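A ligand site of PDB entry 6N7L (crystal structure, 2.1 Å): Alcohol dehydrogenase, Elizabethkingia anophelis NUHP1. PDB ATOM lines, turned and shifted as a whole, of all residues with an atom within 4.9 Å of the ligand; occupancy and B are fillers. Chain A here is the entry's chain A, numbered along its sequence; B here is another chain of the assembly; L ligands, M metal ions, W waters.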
ATOM      1  N   CYS A  51      21.087  11.494  -1.639  1.00  0.00           N
ATOM      2  CA  CYS A  51      22.210  11.772  -0.752  1.00  0.00           C
ATOM      3  C   CYS A  51      21.933  13.071  -0.008  1.00  0.00           C
ATOM      4  O   CYS A  51      21.301  13.983  -0.547  1.00  0.00           O
ATOM      5  CB  CYS A  51      23.504  11.880  -1.557  1.00  0.00           C
ATOM      6  SG  CYS A  51      25.018  12.233  -0.586  1.00  0.00           S
ATOM      7  N   HIS A  52      22.436  13.182   1.227  1.00  0.00           N
ATOM      8  CA  HIS A  52      22.199  14.400   1.998  1.00  0.00           C
ATOM      9  C   HIS A  52      22.827  15.599   1.307  1.00  0.00           C
ATOM     10  O   HIS A  52      22.365  16.730   1.477  1.00  0.00           O
ATOM     11  CB  HIS A  52      22.724  14.234   3.421  1.00  0.00           C
ATOM     12  CG  HIS A  52      22.111  15.158   4.428  1.00  0.00           C
ATOM     13  ND1 HIS A  52      21.339  14.704   5.484  1.00  0.00           N
ATOM     14  CD2 HIS A  52      22.159  16.510   4.556  1.00  0.00           C
ATOM     15  CE1 HIS A  52      20.933  15.736   6.205  1.00  0.00           C
ATOM     16  NE2 HIS A  52      21.421  16.842   5.669  1.00  0.00           N
ATOM     17  N   THR A  53      23.855  15.352   0.495  1.00  0.00           N
ATOM     18  CA  THR A  53      24.420  16.413  -0.335  1.00  0.00           C
ATOM     19  C   THR A  53      23.352  17.046  -1.223  1.00  0.00           C
ATOM     20  O   THR A  53      23.329  18.260  -1.381  1.00  0.00           O
ATOM     21  CB  THR A  53      25.580  15.858  -1.170  1.00  0.00           C
ATOM     22  OG1 THR A  53      26.707  15.624  -0.316  1.00  0.00           O
ATOM     23  CG2 THR A  53      25.987  16.845  -2.253  1.00  0.00           C
ATOM     24  N   HIS A  56      21.744  19.529   0.984  1.00  0.00           N
ATOM     25  CA  HIS A  56      22.609  20.695   1.143  1.00  0.00           C
ATOM     26  C   HIS A  56      22.561  21.568  -0.108  1.00  0.00           C
ATOM     27  O   HIS A  56      22.591  22.801  -0.019  1.00  0.00           O
ATOM     28  CB  HIS A  56      24.054  20.260   1.420  1.00  0.00           C
ATOM     29  CG  HIS A  56      24.267  19.644   2.776  1.00  0.00           C
ATOM     30  ND1 HIS A  56      23.800  20.216   3.935  1.00  0.00           N
ATOM     31  CD2 HIS A  56      24.914  18.516   3.157  1.00  0.00           C
ATOM     32  CE1 HIS A  56      24.128  19.461   4.971  1.00  0.00           C
ATOM     33  NE2 HIS A  56      24.812  18.422   4.521  1.00  0.00           N
ATOM     34  N   TRP A  62      26.066  25.425   1.419  1.00  0.00           N
ATOM     35  CA  TRP A  62      27.513  25.504   1.271  1.00  0.00           C
ATOM     36  C   TRP A  62      27.939  26.841   0.678  1.00  0.00           C
ATOM     37  O   TRP A  62      27.160  27.488  -0.017  1.00  0.00           O
ATOM     38  CB  TRP A  62      28.023  24.370   0.382  1.00  0.00           C
ATOM     39  CG  TRP A  62      27.841  23.028   0.983  1.00  0.00           C
ATOM     40  CD1 TRP A  62      27.589  22.740   2.291  1.00  0.00           C
ATOM     41  CD2 TRP A  62      27.868  21.778   0.288  1.00  0.00           C
ATOM     42  NE1 TRP A  62      27.473  21.374   2.453  1.00  0.00           N
ATOM     43  CE2 TRP A  62      27.635  20.762   1.233  1.00  0.00           C
ATOM     44  CE3 TRP A  62      28.076  21.410  -1.050  1.00  0.00           C
ATOM     45  CZ2 TRP A  62      27.610  19.413   0.895  1.00  0.00           C
ATOM     46  CZ3 TRP A  62      28.051  20.061  -1.388  1.00  0.00           C
ATOM     47  CH2 TRP A  62      27.824  19.080  -0.413  1.00  0.00           C
ATOM     48  N   CYS A 160      27.860   6.927  -4.309  1.00  0.00           N
ATOM     49  CA  CYS A 160      28.367   8.028  -3.501  1.00  0.00           C
ATOM     50  C   CYS A 160      28.559   7.627  -2.047  1.00  0.00           C
ATOM     51  O   CYS A 160      29.683   7.667  -1.538  1.00  0.00           O
ATOM     52  CB  CYS A 160      27.460   9.257  -3.562  1.00  0.00           C
ATOM     53  SG  CYS A 160      28.294  10.686  -2.802  1.00  0.00           S
ATOM     54  N   THR A 164      32.430   6.810  -0.921  1.00  0.00           N
ATOM     55  CA  THR A 164      32.882   7.845   0.001  1.00  0.00           C
ATOM     56  C   THR A 164      33.402   7.253   1.301  1.00  0.00           C
ATOM     57  O   THR A 164      34.512   7.578   1.747  1.00  0.00           O
ATOM     58  CB  THR A 164      31.757   8.826   0.311  1.00  0.00           C
ATOM     59  OG1 THR A 164      31.397   9.562  -0.872  1.00  0.00           O
ATOM     60  CG2 THR A 164      32.189   9.801   1.463  1.00  0.00           C
ATOM     61  N   SER A 183      30.498   7.615  13.097  1.00  0.00           N
ATOM     62  CA  SER A 183      29.613   8.607  13.692  1.00  0.00           C
ATOM     63  C   SER A 183      28.570   9.024  12.674  1.00  0.00           C
ATOM     64  O   SER A 183      28.906   9.591  11.619  1.00  0.00           O
ATOM     65  CB  SER A 183      30.395   9.818  14.212  1.00  0.00           C
ATOM     66  OG  SER A 183      29.534  10.773  14.820  1.00  0.00           O
ATOM     67  N   GLY A 184      27.301   8.733  12.988  1.00  0.00           N
ATOM     68  CA  GLY A 184      26.214   8.984  12.056  1.00  0.00           C
ATOM     69  C   GLY A 184      25.911   7.746  11.236  1.00  0.00           C
ATOM     70  O   GLY A 184      26.600   7.469  10.248  1.00  0.00           O
ATOM     71  N   ILE A 185      24.920   6.964  11.641  1.00  0.00           N
ATOM     72  CA  ILE A 185      24.625   5.748  10.903  1.00  0.00           C
ATOM     73  C   ILE A 185      23.482   6.046   9.929  1.00  0.00           C
ATOM     74  O   ILE A 185      22.397   5.446  10.010  1.00  0.00           O
ATOM     75  CB  ILE A 185      24.282   4.577  11.853  1.00  0.00           C
ATOM     76  CG1 ILE A 185      25.263   4.529  13.050  1.00  0.00           C
ATOM     77  CG2 ILE A 185      24.300   3.257  11.106  1.00  0.00           C
ATOM     78  CD1 ILE A 185      26.763   4.453  12.645  1.00  0.00           C
ATOM     79  N   GLY A 186      23.717   6.963   9.013  1.00  0.00           N
ATOM     80  CA  GLY A 186      22.721   7.298   7.997  1.00  0.00           C
ATOM     81  C   GLY A 186      23.049   6.636   6.684  1.00  0.00           C
ATOM     82  O   GLY A 186      23.586   5.521   6.658  1.00  0.00           O
ATOM     83  N   GLY A 187      22.777   7.337   5.585  1.00  0.00           N
ATOM     84  CA  GLY A 187      23.101   6.789   4.276  1.00  0.00           C
ATOM     85  C   GLY A 187      24.557   6.365   4.167  1.00  0.00           C
ATOM     86  O   GLY A 187      24.866   5.223   3.808  1.00  0.00           O
ATOM     87  N   LEU A 188      25.463   7.273   4.497  1.00  0.00           N
ATOM     88  CA  LEU A 188      26.879   6.916   4.489  1.00  0.00           C
ATOM     89  C   LEU A 188      27.201   5.934   5.606  1.00  0.00           C
ATOM     90  O   LEU A 188      27.855   4.907   5.380  1.00  0.00           O
ATOM     91  CB  LEU A 188      27.722   8.183   4.647  1.00  0.00           C
ATOM     92  CG  LEU A 188      28.128   8.891   3.356  1.00  0.00           C
ATOM     93  CD1 LEU A 188      26.912   9.466   2.616  1.00  0.00           C
ATOM     94  CD2 LEU A 188      29.125   9.976   3.689  1.00  0.00           C
ATOM     95  N   GLY A 189      26.728   6.224   6.815  1.00  0.00           N
ATOM     96  CA  GLY A 189      27.198   5.479   7.969  1.00  0.00           C
ATOM     97  C   GLY A 189      26.850   4.003   7.936  1.00  0.00           C
ATOM     98  O   GLY A 189      27.647   3.161   8.375  1.00  0.00           O
ATOM     99  N   ILE A 206      28.057   5.351  16.482  1.00  0.00           N
ATOM    100  CA  ILE A 206      27.594   6.488  17.269  1.00  0.00           C
ATOM    101  C   ILE A 206      26.464   7.177  16.512  1.00  0.00           C
ATOM    102  O   ILE A 206      26.609   7.503  15.318  1.00  0.00           O
ATOM    103  CB  ILE A 206      28.727   7.491  17.541  1.00  0.00           C
ATOM    104  CG1 ILE A 206      29.896   6.827  18.274  1.00  0.00           C
ATOM    105  CG2 ILE A 206      28.216   8.660  18.356  1.00  0.00           C
ATOM    106  CD1 ILE A 206      31.194   7.586  18.141  1.00  0.00           C
ATOM    107  N   ASP A 207      25.357   7.415  17.192  1.00  0.00           N
ATOM    108  CA  ASP A 207      24.308   8.254  16.621  1.00  0.00           C
ATOM    109  C   ASP A 207      23.521   8.832  17.790  1.00  0.00           C
ATOM    110  O   ASP A 207      23.916   8.696  18.952  1.00  0.00           O
ATOM    111  CB  ASP A 207      23.442   7.479  15.620  1.00  0.00           C
ATOM    112  CG  ASP A 207      22.881   8.374  14.512  1.00  0.00           C
ATOM    113  OD1 ASP A 207      22.209   9.368  14.840  1.00  0.00           O
ATOM    114  OD2 ASP A 207      23.076   8.072  13.309  1.00  0.00           O
ATOM    115  N   VAL A 208      22.390   9.475  17.478  1.00  0.00           N
ATOM    116  CA  VAL A 208      21.601  10.171  18.469  1.00  0.00           C
ATOM    117  C   VAL A 208      20.182   9.621  18.555  1.00  0.00           C
ATOM    118  O   VAL A 208      19.309  10.271  19.096  1.00  0.00           O
ATOM    119  CB  VAL A 208      21.579  11.696  18.200  1.00  0.00           C
ATOM    120  CG1 VAL A 208      22.957  12.295  18.407  1.00  0.00           C
ATOM    121  CG2 VAL A 208      21.074  11.981  16.783  1.00  0.00           C
ATOM    122  N   LYS A 212      18.821   4.152  14.826  1.00  0.00           N
ATOM    123  CA  LYS A 212      20.038   4.175  14.015  1.00  0.00           C
ATOM    124  C   LYS A 212      21.059   3.159  14.529  1.00  0.00           C
ATOM    125  O   LYS A 212      21.760   2.514  13.741  1.00  0.00           O
ATOM    126  CB  LYS A 212      20.630   5.581  14.011  1.00  0.00           C
ATOM    127  CG  LYS A 212      19.661   6.656  13.565  1.00  0.00           C
ATOM    128  CD  LYS A 212      19.446   6.562  12.078  1.00  0.00           C
ATOM    129  CE  LYS A 212      18.643   7.723  11.531  1.00  0.00           C
ATOM    130  NZ  LYS A 212      18.820   7.767  10.053  1.00  0.00           N
ATOM    131  N   ALA A 227      24.737   9.111  21.557  1.00  0.00           N
ATOM    132  CA  ALA A 227      25.439  10.286  22.073  1.00  0.00           C
ATOM    133  C   ALA A 227      24.532  11.197  22.877  1.00  0.00           C
ATOM    134  O   ALA A 227      25.028  12.007  23.661  1.00  0.00           O
ATOM    135  CB  ALA A 227      26.099  11.060  20.926  1.00  0.00           C
ATOM    136  N   THR A 249      30.412  10.842   9.570  1.00  0.00           N
ATOM    137  CA  THR A 249      29.434  11.048   8.513  1.00  0.00           C
ATOM    138  C   THR A 249      28.236  11.852   8.995  1.00  0.00           C
ATOM    139  O   THR A 249      27.266  12.010   8.242  1.00  0.00           O
ATOM    140  CB  THR A 249      28.985   9.690   7.966  1.00  0.00           C
ATOM    141  OG1 THR A 249      28.224   9.001   8.960  1.00  0.00           O
ATOM    142  CG2 THR A 249      30.194   8.829   7.607  1.00  0.00           C
ATOM    143  N   ALA A 250      28.282  12.397  10.202  1.00  0.00           N
ATOM    144  CA  ALA A 250      27.140  13.063  10.809  1.00  0.00           C
ATOM    145  C   ALA A 250      27.002  14.496  10.283  1.00  0.00           C
ATOM    146  O   ALA A 250      27.931  15.068   9.715  1.00  0.00           O
ATOM    147  CB  ALA A 250      27.274  13.057  12.324  1.00  0.00           C
ATOM    148  N   VAL A 251      25.823  15.069  10.497  1.00  0.00           N
ATOM    149  CA  VAL A 251      25.480  16.376   9.936  1.00  0.00           C
ATOM    150  C   VAL A 251      25.411  17.448  11.015  1.00  0.00           C
ATOM    151  O   VAL A 251      24.629  18.412  10.903  1.00  0.00           O
ATOM    152  CB  VAL A 251      24.166  16.285   9.143  1.00  0.00           C
ATOM    153  CG1 VAL A 251      24.392  15.560   7.813  1.00  0.00           C
ATOM    154  CG2 VAL A 251      23.094  15.535   9.961  1.00  0.00           C
ATOM    155  N   SER A 252      26.210  17.306  12.085  1.00  0.00           N
ATOM    156  CA  SER A 252      26.176  18.269  13.181  1.00  0.00           C
ATOM    157  C   SER A 252      27.608  18.476  13.689  1.00  0.00           C
ATOM    158  O   SER A 252      28.347  17.474  13.859  1.00  0.00           O
ATOM    159  CB  SER A 252      25.256  17.793  14.311  1.00  0.00           C
ATOM    160  OG  SER A 252      25.306  18.685  15.429  1.00  0.00           O
ATOM    161  N   ILE A 254      28.952  19.086  16.588  1.00  0.00           N
ATOM    162  CA  ILE A 254      29.315  18.457  17.858  1.00  0.00           C
ATOM    163  C   ILE A 254      29.750  17.001  17.649  1.00  0.00           C
ATOM    164  O   ILE A 254      30.551  16.466  18.422  1.00  0.00           O
ATOM    165  CB  ILE A 254      28.160  18.566  18.873  1.00  0.00           C
ATOM    166  CG1 ILE A 254      28.579  18.040  20.252  1.00  0.00           C
ATOM    167  CG2 ILE A 254      26.929  17.825  18.397  1.00  0.00           C
ATOM    168  CD1 ILE A 254      29.757  18.779  20.853  1.00  0.00           C
ATOM    169  N   ALA A 255      29.231  16.346  16.599  1.00  0.00           N
ATOM    170  CA  ALA A 255      29.679  14.980  16.302  1.00  0.00           C
ATOM    171  C   ALA A 255      31.151  14.936  15.940  1.00  0.00           C
ATOM    172  O   ALA A 255      31.837  13.931  16.192  1.00  0.00           O
ATOM    173  CB  ALA A 255      28.867  14.384  15.158  1.00  0.00           C
ATOM    174  N   LEU A 271      37.035  12.894   7.945  1.00  0.00           N
ATOM    175  CA  LEU A 271      35.809  13.689   7.916  1.00  0.00           C
ATOM    176  C   LEU A 271      35.123  13.520   6.564  1.00  0.00           C
ATOM    177  O   LEU A 271      35.700  13.877   5.534  1.00  0.00           O
ATOM    178  CB  LEU A 271      36.094  15.158   8.195  1.00  0.00           C
ATOM    179  CG  LEU A 271      36.878  15.509   9.461  1.00  0.00           C
ATOM    180  CD1 LEU A 271      36.990  17.041   9.644  1.00  0.00           C
ATOM    181  CD2 LEU A 271      36.217  14.842  10.685  1.00  0.00           C
ATOM    182  N   ASN A 272      33.884  13.004   6.576  1.00  0.00           N
ATOM    183  CA  ASN A 272      33.002  12.988   5.416  1.00  0.00           C
ATOM    184  C   ASN A 272      31.860  13.990   5.530  1.00  0.00           C
ATOM    185  O   ASN A 272      31.525  14.648   4.538  1.00  0.00           O
ATOM    186  CB  ASN A 272      32.375  11.597   5.198  1.00  0.00           C
ATOM    187  CG  ASN A 272      33.344  10.570   4.635  1.00  0.00           C
ATOM    188  OD1 ASN A 272      33.095   9.385   4.764  1.00  0.00           O
ATOM    189  ND2 ASN A 272      34.426  11.016   3.977  1.00  0.00           N
ATOM    190  N   GLY A 273      31.256  14.106   6.708  1.00  0.00           N
ATOM    191  CA  GLY A 273      30.059  14.928   6.838  1.00  0.00           C
ATOM    192  C   GLY A 273      30.325  16.372   6.464  1.00  0.00           C
ATOM    193  O   GLY A 273      31.420  16.902   6.676  1.00  0.00           O
ATOM    194  N   LEU A 274      29.296  17.018   5.892  1.00  0.00           N
ATOM    195  CA  LEU A 274      29.446  18.364   5.367  1.00  0.00           C
ATOM    196  C   LEU A 274      28.378  19.342   5.879  1.00  0.00           C
ATOM    197  O   LEU A 274      27.800  20.106   5.105  1.00  0.00           O
ATOM    198  CB  LEU A 274      29.430  18.310   3.840  1.00  0.00           C
ATOM    199  CG  LEU A 274      30.694  17.748   3.170  1.00  0.00           C
ATOM    200  CD1 LEU A 274      30.446  17.465   1.658  1.00  0.00           C
ATOM    201  CD2 LEU A 274      31.871  18.711   3.340  1.00  0.00           C
ATOM    202  N   PRO A 275      28.170  19.413   7.200  1.00  0.00           N
ATOM    203  CA  PRO A 275      27.299  20.467   7.718  1.00  0.00           C
ATOM    204  C   PRO A 275      27.953  21.824   7.521  1.00  0.00           C
ATOM    205  O   PRO A 275      29.192  21.928   7.480  1.00  0.00           O
ATOM    206  CB  PRO A 275      27.178  20.120   9.211  1.00  0.00           C
ATOM    207  CG  PRO A 275      28.522  19.516   9.521  1.00  0.00           C
ATOM    208  CD  PRO A 275      28.830  18.680   8.297  1.00  0.00           C
ATOM    209  N   SER A 296      38.018  13.986   3.828  1.00  0.00           N
ATOM    210  CA  SER A 296      37.990  12.951   2.806  1.00  0.00           C
ATOM    211  C   SER A 296      36.805  13.189   1.877  1.00  0.00           C
ATOM    212  O   SER A 296      35.671  13.299   2.343  1.00  0.00           O
ATOM    213  CB  SER A 296      37.926  11.542   3.416  1.00  0.00           C
ATOM    214  OG  SER A 296      38.135  10.538   2.437  1.00  0.00           O
ATOM    215  N   ILE A 297      37.070  13.263   0.571  1.00  0.00           N
ATOM    216  CA  ILE A 297      36.083  13.711  -0.403  1.00  0.00           C
ATOM    217  C   ILE A 297      35.895  12.611  -1.454  1.00  0.00           C
ATOM    218  O   ILE A 297      36.805  12.318  -2.246  1.00  0.00           O
ATOM    219  CB  ILE A 297      36.456  15.066  -1.019  1.00  0.00           C
ATOM    220  CG1 ILE A 297      35.477  15.456  -2.125  1.00  0.00           C
ATOM    221  CG2 ILE A 297      37.931  15.106  -1.477  1.00  0.00           C
ATOM    222  CD1 ILE A 297      34.030  15.677  -1.630  1.00  0.00           C
ATOM    223  N   VAL A 298      34.684  12.035  -1.475  1.00  0.00           N
ATOM    224  CA  VAL A 298      34.271  10.899  -2.307  1.00  0.00           C
ATOM    225  C   VAL A 298      35.442   9.936  -2.559  1.00  0.00           C
ATOM    226  O   VAL A 298      36.141   9.567  -1.607  1.00  0.00           O
ATOM    227  CB  VAL A 298      33.583  11.384  -3.611  1.00  0.00           C
ATOM    228  CG1 VAL A 298      32.272  12.132  -3.239  1.00  0.00           C
ATOM    229  CG2 VAL A 298      34.476  12.283  -4.479  1.00  0.00           C
ATOM    230  N   MET A 335      14.323  13.055   5.557  1.00  0.00           N
ATOM    231  CA  MET A 335      15.750  13.189   5.779  1.00  0.00           C
ATOM    232  C   MET A 335      16.041  14.252   6.834  1.00  0.00           C
ATOM    233  O   MET A 335      16.862  14.023   7.734  1.00  0.00           O
ATOM    234  CB  MET A 335      16.472  13.510   4.472  1.00  0.00           C
ATOM    235  CG  MET A 335      17.990  13.614   4.596  1.00  0.00           C
ATOM    236  SD  MET A 335      18.781  13.820   2.986  1.00  0.00           S
ATOM    237  CE  MET A 335      18.940  12.114   2.446  1.00  0.00           C
ATOM    238  N   GLY A 342      18.700   4.045   6.636  1.00  0.00           N
ATOM    239  CA  GLY A 342      19.716   3.919   5.618  1.00  0.00           C
ATOM    240  C   GLY A 342      19.559   4.915   4.495  1.00  0.00           C
ATOM    241  O   GLY A 342      19.798   6.111   4.689  1.00  0.00           O
ATOM    242  N   ARG A 343      19.148   4.450   3.325  1.00  0.00           N
ATOM    243  CA  ARG A 343      19.046   5.278   2.125  1.00  0.00           C
ATOM    244  C   ARG A 343      17.646   5.174   1.533  1.00  0.00           C
ATOM    245  O   ARG A 343      17.025   4.118   1.564  1.00  0.00           O
ATOM    246  CB  ARG A 343      20.069   4.831   1.055  1.00  0.00           C
ATOM    247  CG  ARG A 343      21.361   5.676   0.967  1.00  0.00           C
ATOM    248  CD  ARG A 343      21.130   6.966   0.196  1.00  0.00           C
ATOM    249  NE  ARG A 343      22.373   7.606  -0.208  1.00  0.00           N
ATOM    250  CZ  ARG A 343      23.025   8.488   0.532  1.00  0.00           C
ATOM    251  NH1 ARG A 343      22.549   8.863   1.712  1.00  0.00           N
ATOM    252  NH2 ARG A 343      24.149   9.025   0.074  1.00  0.00           N
ATOM    253  N   VAL B 287      37.152  19.168   4.229  1.00  0.00           N
ATOM    254  CA  VAL B 287      36.756  17.939   3.527  1.00  0.00           C
ATOM    255  C   VAL B 287      37.077  18.035   2.041  1.00  0.00           C
ATOM    256  O   VAL B 287      37.751  17.153   1.482  1.00  0.00           O
ATOM    257  CB  VAL B 287      35.266  17.657   3.750  1.00  0.00           C
ATOM    258  CG1 VAL B 287      34.807  16.495   2.839  1.00  0.00           C
ATOM    259  CG2 VAL B 287      35.009  17.364   5.230  1.00  0.00           C
HETATM  260  P1  LIG L   1      21.863  11.121   6.346  1.00  0.00           P
HETATM  261  O1  LIG L   1      21.351   9.909   5.676  1.00  0.00           O
HETATM  262  O2  LIG L   1      20.836  12.207   6.570  1.00  0.00           O
HETATM  263  O3  LIG L   1      22.459  10.723   7.770  1.00  0.00           O
HETATM  264  C1  LIG L   1      22.980  11.653   8.740  1.00  0.00           C
HETATM  265  C2  LIG L   1      23.105  10.859  10.018  1.00  0.00           C
HETATM  266  O4  LIG L   1      23.781  11.635  11.034  1.00  0.00           O
HETATM  267  C3  LIG L   1      21.780  10.390  10.635  1.00  0.00           C
HETATM  268  O5  LIG L   1      21.840   8.997  10.914  1.00  0.00           O
HETATM  269  C4  LIG L   1      21.693  11.210  11.928  1.00  0.00           C
HETATM  270  O6  LIG L   1      20.972  10.532  12.950  1.00  0.00           O
HETATM  271  C5  LIG L   1      23.171  11.312  12.258  1.00  0.00           C
HETATM  272  N1  LIG L   1      23.515  12.321  13.240  1.00  0.00           N
HETATM  273  C6  LIG L   1      22.952  13.567  13.416  1.00  0.00           C
HETATM  274  N2  LIG L   1      23.445  14.238  14.433  1.00  0.00           N
HETATM  275  C7  LIG L   1      24.402  13.377  14.962  1.00  0.00           C
HETATM  276  C8  LIG L   1      25.283  13.505  16.051  1.00  0.00           C
HETATM  277  N3  LIG L   1      25.332  14.572  16.853  1.00  0.00           N
HETATM  278  N4  LIG L   1      26.120  12.467  16.290  1.00  0.00           N
HETATM  279  C9  LIG L   1      26.067  11.394  15.500  1.00  0.00           C
HETATM  280  N5  LIG L   1      25.268  11.159  14.454  1.00  0.00           N
HETATM  281  C10 LIG L   1      24.456  12.210  14.238  1.00  0.00           C
HETATM  282  O7  LIG L   1      22.998  11.788   5.451  1.00  0.00           O
HETATM  283  P2  LIG L   1      24.075  11.132   4.474  1.00  0.00           P
HETATM  284  O8  LIG L   1      23.517  11.017   3.109  1.00  0.00           O
HETATM  285  O9  LIG L   1      24.644   9.934   5.136  1.00  0.00           O
HETATM  286  O10 LIG L   1      25.150  12.306   4.419  1.00  0.00           O
HETATM  287  C11 LIG L   1      25.848  12.692   5.610  1.00  0.00           C
HETATM  288  C12 LIG L   1      26.736  13.881   5.325  1.00  0.00           C
HETATM  289  O11 LIG L   1      27.861  13.477   4.507  1.00  0.00           O
HETATM  290  C13 LIG L   1      26.078  15.063   4.610  1.00  0.00           C
HETATM  291  O12 LIG L   1      26.661  16.262   5.126  1.00  0.00           O
HETATM  292  C14 LIG L   1      26.526  14.866   3.168  1.00  0.00           C
HETATM  293  O13 LIG L   1      26.532  16.065   2.404  1.00  0.00           O
HETATM  294  C15 LIG L   1      27.945  14.355   3.410  1.00  0.00           C
HETATM  295  N6  LIG L   1      28.563  13.593   2.235  1.00  0.00           N
HETATM  296  C16 LIG L   1      29.862  13.833   2.037  1.00  0.00           C
HETATM  297  C17 LIG L   1      30.563  13.151   1.068  1.00  0.00           C
HETATM  298  C18 LIG L   1      32.070  13.269   0.952  1.00  0.00           C
HETATM  299  O14 LIG L   1      32.634  12.817  -0.049  1.00  0.00           O
HETATM  300  N7  LIG L   1      32.720  13.940   1.901  1.00  0.00           N
HETATM  301  C19 LIG L   1      29.866  12.222   0.279  1.00  0.00           C
HETATM  302  C20 LIG L   1      28.521  11.986   0.515  1.00  0.00           C
HETATM  303  C21 LIG L   1      27.876  12.692   1.507  1.00  0.00           C
HETATM  304 ZN    ZN M   1      26.735  12.357  -2.225  1.00  0.00          ZN
HETATM  305  O   HOH W   1      28.435  12.410  18.399  1.00  0.00           O
HETATM  306  O   HOH W   2      19.608   8.223   6.939  1.00  0.00           O
HETATM  307  O   HOH W   3      18.673  11.992   8.165  1.00  0.00           O
HETATM  308  O   HOH W   4      20.123   8.728   3.563  1.00  0.00           O
HETATM  309  O   HOH W   5      25.455   8.675   7.560  1.00  0.00           O
HETATM  310  O   HOH W   6      28.168  13.988  -1.899  1.00  0.00           O
HETATM  311  O   HOH W   7      23.534  16.899  17.115  1.00  0.00           O
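An oxygen (O6) of the ligand sits at hydrogen-bond distance from the side-chain carboxylate (OD1) of Asp 207, 2.5 Å away. The backbone NH (N) of Val 298 is in hydrogen-bond range of an oxygen (O14) of the ligand (2.6 Å). O8 of the ligand lies within salt-bridge range of NH1 of Arg 343. N of Thr 53 lies within hydrogen-bond range of O13 of the ligand, at 3.4 Å. OG1 of Thr 53 is in hydrogen-bond range of O13 of the ligand (2.8 Å). The backbone NH of His 52 lies within hydrogen-bond range of an oxygen (O8) of the ligand (3.1 Å). ND1 of His 52 is in hydrogen-bond range of O2 of the ligand, 2.8 Å away. N of Leu 274 sits at hydrogen-bond distance from O12 of the ligand (2.8 Å). N of Leu 188 is in hydrogen-bond range of O9 of the ligand, at 2.9 Å. An oxygen (O12) of the ligand sits at hydrogen-bond distance from a ring nitrogen (NE2) of His 56 (2.9 Å). N of Gly 187 sits at hydrogen-bond distance from O1 of the ligand, 2.9 Å away. O of Asn 272 is in hydrogen-bond range of N7 of the ligand, at 3.0 Å. The backbone carbonyl oxygen (O) of Ser 296 lies within hydrogen-bond range of a nitrogen (N7) of the ligand, at 3.1 Å. N of Gly 186 sits at hydrogen-bond distance from O5 of the ligand (3.4 Å). The side-chain amino group of Lys 212 sits at hydrogen-bond distance from an oxygen (O5) of the ligand. N5 of the ligand lies close to N of Gly 184, at 3.5 Å.
SG of Cys 51 touches C21 of the ligand, 3.6 Å away. Trp 62 touches the ligand (CZ2 to O13, 3.8 Å). Cys 160 touches the ligand (SG to C20, 3.6 Å). Thr 164 touches the ligand. Ser 183 touches the ligand (OG to C9, 3.6 Å). Ile 185 touches the ligand. Ile 206 touches the ligand. CG1 of Val 208 touches C8 of the ligand, at 3.5 Å. Thr 249 touches the ligand (O to C11, 3.1 Å). CB of Ala 250 touches N5 of the ligand, 3.5 Å away. Val 251 touches the ligand. Ser 252 touches the ligand (CB to N2, 3.99 Å). Ile 254 touches the ligand. Ala 255 touches the ligand. Gly 273 touches the ligand. Ile 297 touches the ligand. Met 335 touches the ligand (CG to O2, 3.7 Å). Val 287 of chain B touches the ligand.
Water W3 bridges an oxygen (O2) of the ligand (2.7 Å) and the backbone carbonyl oxygen (O) of Met 335 (2.8 Å). Water W4 lies within hydrogen-bond range of O1 of the ligand, O of Gly 342 and NH1 of Arg 343. Water W2 lies within hydrogen-bond range of an oxygen (O1) of the ligand (2.7 Å), the backbone carbonyl oxygen (O) of Gly 342 (3.1 Å) and the side-chain amino group (NZ) of Lys 212 (3.2 Å). Water W7 bridges N3 of the ligand and OG of Ser 252.
The backbone carbonyl oxygen (O) of Asp 207 is in hydrogen-bond range of the backbone NH (N) of Ala 227, 2.8 Å away. The guanidinium group (NH2) of Arg 343 sits close to the side-chain sulfur (SG) of Cys 51, 3.4 Å away. A ring nitrogen (ND1) of His 52 sits close to the side-chain sulfur (SD) of Met 335, 3.7 Å away. O of Leu 274 is in hydrogen-bond range of NE2 of His 56, at 3.5 Å. The backbone carbonyl oxygen of Leu 274 sits at hydrogen-bond distance from the indole nitrogen of Trp 62 (3.0 Å). The side-chain amide nitrogen (ND2) of Asn 272 is in hydrogen-bond range of the backbone carbonyl oxygen (O) of Ser 296, at 3.1 Å. O of Leu 271 is in hydrogen-bond range of N of Ser 296, at 2.9 Å. OG1 of Thr 249 sits at hydrogen-bond distance from O of Ser 183, at 2.8 Å.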
